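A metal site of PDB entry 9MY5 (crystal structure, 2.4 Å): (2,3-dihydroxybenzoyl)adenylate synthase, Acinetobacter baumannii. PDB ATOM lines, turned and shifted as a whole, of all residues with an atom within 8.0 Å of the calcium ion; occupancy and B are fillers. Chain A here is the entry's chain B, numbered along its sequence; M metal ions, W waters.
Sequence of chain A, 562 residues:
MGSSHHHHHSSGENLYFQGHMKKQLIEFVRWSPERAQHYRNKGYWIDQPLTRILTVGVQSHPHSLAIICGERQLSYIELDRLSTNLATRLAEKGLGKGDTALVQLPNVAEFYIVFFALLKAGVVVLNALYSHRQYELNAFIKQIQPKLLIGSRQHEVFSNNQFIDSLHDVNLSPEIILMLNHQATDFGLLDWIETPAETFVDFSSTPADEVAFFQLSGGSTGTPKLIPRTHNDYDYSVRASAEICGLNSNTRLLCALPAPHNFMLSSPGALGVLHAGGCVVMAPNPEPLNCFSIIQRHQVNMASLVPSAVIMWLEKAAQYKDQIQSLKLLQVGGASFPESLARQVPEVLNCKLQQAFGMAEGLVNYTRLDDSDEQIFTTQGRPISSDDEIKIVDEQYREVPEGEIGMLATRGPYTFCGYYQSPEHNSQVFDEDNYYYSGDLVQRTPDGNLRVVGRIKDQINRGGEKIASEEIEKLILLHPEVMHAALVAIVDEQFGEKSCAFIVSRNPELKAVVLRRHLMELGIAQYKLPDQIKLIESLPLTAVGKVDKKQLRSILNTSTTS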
ATOM      1  N   VAL A 300      19.154  16.881 -28.049  1.00  0.00           N
ATOM      2  CA  VAL A 300      18.784  15.877 -27.051  1.00  0.00           C
ATOM      3  C   VAL A 300      17.824  16.491 -26.035  1.00  0.00           C
ATOM      4  O   VAL A 300      18.044  17.618 -25.565  1.00  0.00           O
ATOM      5  CB  VAL A 300      20.059  15.330 -26.374  1.00  0.00           C
ATOM      6  CG1 VAL A 300      19.694  14.530 -25.150  1.00  0.00           C
ATOM      7  CG2 VAL A 300      20.860  14.491 -27.369  1.00  0.00           C
ATOM      8  N   ASN A 301      16.739  15.772 -25.705  1.00  0.00           N
ATOM      9  CA  ASN A 301      15.826  16.298 -24.705  1.00  0.00           C
ATOM     10  C   ASN A 301      15.684  15.413 -23.474  1.00  0.00           C
ATOM     11  O   ASN A 301      14.903  15.746 -22.582  1.00  0.00           O
ATOM     12  CB  ASN A 301      14.435  16.592 -25.308  1.00  0.00           C
ATOM     13  CG  ASN A 301      13.870  15.429 -26.074  1.00  0.00           C
ATOM     14  OD1 ASN A 301      14.143  14.267 -25.762  1.00  0.00           O
ATOM     15  ND2 ASN A 301      13.064  15.727 -27.088  1.00  0.00           N
ATOM     16  N   LYS A 321      25.211  26.732 -20.591  1.00  0.00           N
ATOM     17  CA  LYS A 321      23.755  26.777 -20.567  1.00  0.00           C
ATOM     18  C   LYS A 321      23.172  26.599 -21.960  1.00  0.00           C
ATOM     19  O   LYS A 321      22.228  25.818 -22.140  1.00  0.00           O
ATOM     20  CB  LYS A 321      23.250  28.075 -19.954  1.00  0.00           C
ATOM     21  CG  LYS A 321      23.082  28.039 -18.451  1.00  0.00           C
ATOM     22  CD  LYS A 321      22.968  29.458 -17.899  1.00  0.00           C
ATOM     23  N   ILE A 324      23.044  23.044 -23.616  1.00  0.00           N
ATOM     24  CA  ILE A 324      22.209  22.027 -23.016  1.00  0.00           C
ATOM     25  C   ILE A 324      20.771  22.499 -22.801  1.00  0.00           C
ATOM     26  O   ILE A 324      19.993  21.803 -22.154  1.00  0.00           O
ATOM     27  CB  ILE A 324      22.827  21.495 -21.705  1.00  0.00           C
ATOM     28  CG1 ILE A 324      22.715  22.521 -20.590  1.00  0.00           C
ATOM     29  CG2 ILE A 324      24.291  21.136 -21.903  1.00  0.00           C
ATOM     30  CD1 ILE A 324      22.874  21.883 -19.244  1.00  0.00           C
ATOM     31  N   GLN A 325      20.382  23.659 -23.348  1.00  0.00           N
ATOM     32  CA  GLN A 325      19.036  24.174 -23.092  1.00  0.00           C
ATOM     33  C   GLN A 325      17.948  23.157 -23.459  1.00  0.00           C
ATOM     34  O   GLN A 325      16.945  23.021 -22.734  1.00  0.00           O
ATOM     35  CB  GLN A 325      18.798  25.472 -23.861  1.00  0.00           C
ATOM     36  CG  GLN A 325      19.018  25.370 -25.377  1.00  0.00           C
ATOM     37  CD  GLN A 325      18.751  26.695 -26.109  1.00  0.00           C
ATOM     38  OE1 GLN A 325      18.882  26.781 -27.350  1.00  0.00           O
ATOM     39  NE2 GLN A 325      18.397  27.719 -25.351  1.00  0.00           N
ATOM     40  N   SER A 326      18.119  22.438 -24.576  1.00  0.00           N
ATOM     41  CA  SER A 326      17.069  21.541 -25.071  1.00  0.00           C
ATOM     42  C   SER A 326      16.802  20.376 -24.133  1.00  0.00           C
ATOM     43  O   SER A 326      15.788  19.669 -24.314  1.00  0.00           O
ATOM     44  CB  SER A 326      17.431  20.994 -26.462  1.00  0.00           C
ATOM     45  OG  SER A 326      18.451  20.013 -26.353  1.00  0.00           O
ATOM     46  N   LEU A 327      17.658  20.139 -23.158  1.00  0.00           N
ATOM     47  CA  LEU A 327      17.395  19.103 -22.176  1.00  0.00           C
ATOM     48  C   LEU A 327      16.075  19.379 -21.474  1.00  0.00           C
ATOM     49  O   LEU A 327      15.824  20.501 -21.012  1.00  0.00           O
ATOM     50  CB  LEU A 327      18.528  19.048 -21.174  1.00  0.00           C
ATOM     51  CG  LEU A 327      18.909  17.727 -20.539  1.00  0.00           C
ATOM     52  CD1 LEU A 327      18.899  16.669 -21.615  1.00  0.00           C
ATOM     53  CD2 LEU A 327      20.304  17.887 -19.972  1.00  0.00           C
ATOM     54  N   LYS A 328      15.198  18.368 -21.431  1.00  0.00           N
ATOM     55  CA  LYS A 328      13.904  18.498 -20.782  1.00  0.00           C
ATOM     56  C   LYS A 328      13.749  17.645 -19.540  1.00  0.00           C
ATOM     57  O   LYS A 328      12.959  17.994 -18.661  1.00  0.00           O
ATOM     58  CB  LYS A 328      12.791  18.141 -21.771  1.00  0.00           C
ATOM     59  CG  LYS A 328      12.423  19.241 -22.734  1.00  0.00           C
ATOM     60  CD  LYS A 328      11.079  18.935 -23.422  1.00  0.00           C
ATOM     61  CE  LYS A 328      11.152  19.440 -24.851  1.00  0.00           C
ATOM     62  NZ  LYS A 328      12.429  20.266 -25.055  1.00  0.00           N
ATOM     63  N   LEU A 329      14.460  16.528 -19.444  1.00  0.00           N
ATOM     64  CA  LEU A 329      14.195  15.590 -18.370  1.00  0.00           C
ATOM     65  C   LEU A 329      15.446  14.768 -18.089  1.00  0.00           C
ATOM     66  O   LEU A 329      16.057  14.235 -19.021  1.00  0.00           O
ATOM     67  CB  LEU A 329      13.000  14.672 -18.731  1.00  0.00           C
ATOM     68  CG  LEU A 329      12.733  13.512 -17.779  1.00  0.00           C
ATOM     69  CD1 LEU A 329      12.371  14.059 -16.388  1.00  0.00           C
ATOM     70  CD2 LEU A 329      11.643  12.529 -18.294  1.00  0.00           C
ATOM     71  N   PRO A 346      17.263  21.131 -11.629  1.00  0.00           N
ATOM     72  CA  PRO A 346      16.458  22.164 -12.285  1.00  0.00           C
ATOM     73  C   PRO A 346      17.115  23.527 -12.296  1.00  0.00           C
ATOM     74  O   PRO A 346      16.963  24.259 -13.285  1.00  0.00           O
ATOM     75  CB  PRO A 346      15.142  22.155 -11.479  1.00  0.00           C
ATOM     76  CG  PRO A 346      15.420  21.399 -10.231  1.00  0.00           C
ATOM     77  CD  PRO A 346      16.563  20.476 -10.511  1.00  0.00           C
ATOM     78  N   LEU A 349      21.087  22.698 -14.479  1.00  0.00           N
ATOM     79  CA  LEU A 349      20.913  22.002 -15.747  1.00  0.00           C
ATOM     80  C   LEU A 349      19.626  22.379 -16.483  1.00  0.00           C
ATOM     81  O   LEU A 349      19.457  21.988 -17.643  1.00  0.00           O
ATOM     82  CB  LEU A 349      20.965  20.490 -15.540  1.00  0.00           C
ATOM     83  CG  LEU A 349      22.247  19.932 -14.919  1.00  0.00           C
ATOM     84  CD1 LEU A 349      22.083  18.422 -14.650  1.00  0.00           C
ATOM     85  CD2 LEU A 349      23.432  20.223 -15.821  1.00  0.00           C
ATOM     86  N   ASN A 350      18.736  23.132 -15.844  1.00  0.00           N
ATOM     87  CA  ASN A 350      17.563  23.721 -16.511  1.00  0.00           C
ATOM     88  C   ASN A 350      16.676  22.638 -17.141  1.00  0.00           C
ATOM     89  O   ASN A 350      16.225  22.744 -18.297  1.00  0.00           O
ATOM     90  CB  ASN A 350      18.002  24.765 -17.540  1.00  0.00           C
ATOM     91  CG  ASN A 350      18.755  25.922 -16.901  1.00  0.00           C
ATOM     92  OD1 ASN A 350      18.523  26.248 -15.745  1.00  0.00           O
ATOM     93  ND2 ASN A 350      19.666  26.540 -17.654  1.00  0.00           N
ATOM     94  N   CYS A 351      16.379  21.602 -16.369  1.00  0.00           N
ATOM     95  CA  CYS A 351      15.467  20.569 -16.813  1.00  0.00           C
ATOM     96  C   CYS A 351      14.822  19.914 -15.592  1.00  0.00           C
ATOM     97  O   CYS A 351      15.371  19.969 -14.483  1.00  0.00           O
ATOM     98  CB  CYS A 351      16.188  19.523 -17.654  1.00  0.00           C
ATOM     99  SG  CYS A 351      17.396  18.648 -16.629  1.00  0.00           S
ATOM    100  N   LYS A 352      13.682  19.277 -15.808  1.00  0.00           N
ATOM    101  CA  LYS A 352      13.015  18.535 -14.750  1.00  0.00           C
ATOM    102  C   LYS A 352      13.904  17.393 -14.246  1.00  0.00           C
ATOM    103  O   LYS A 352      14.706  16.832 -14.989  1.00  0.00           O
ATOM    104  CB  LYS A 352      11.686  17.956 -15.243  1.00  0.00           C
ATOM    105  CG  LYS A 352      10.910  17.199 -14.181  1.00  0.00           C
ATOM    106  CD  LYS A 352       9.398  17.448 -14.274  1.00  0.00           C
ATOM    107  CE  LYS A 352       8.669  17.099 -12.949  1.00  0.00           C
ATOM    108  NZ  LYS A 352       7.884  18.253 -12.370  1.00  0.00           N
HETATM  109 CA    CA M   1      15.943  22.659 -20.662  1.00  0.00          CA
HETATM  110  O   HOH W   1      18.291  22.517 -20.299  1.00  0.00           O
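Water W1 bridges O of Ile 324 and O of Leu 349.
The calcium ion is bound by O of Leu 327, O of Gln 325, water W1 and O of Asn 350.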
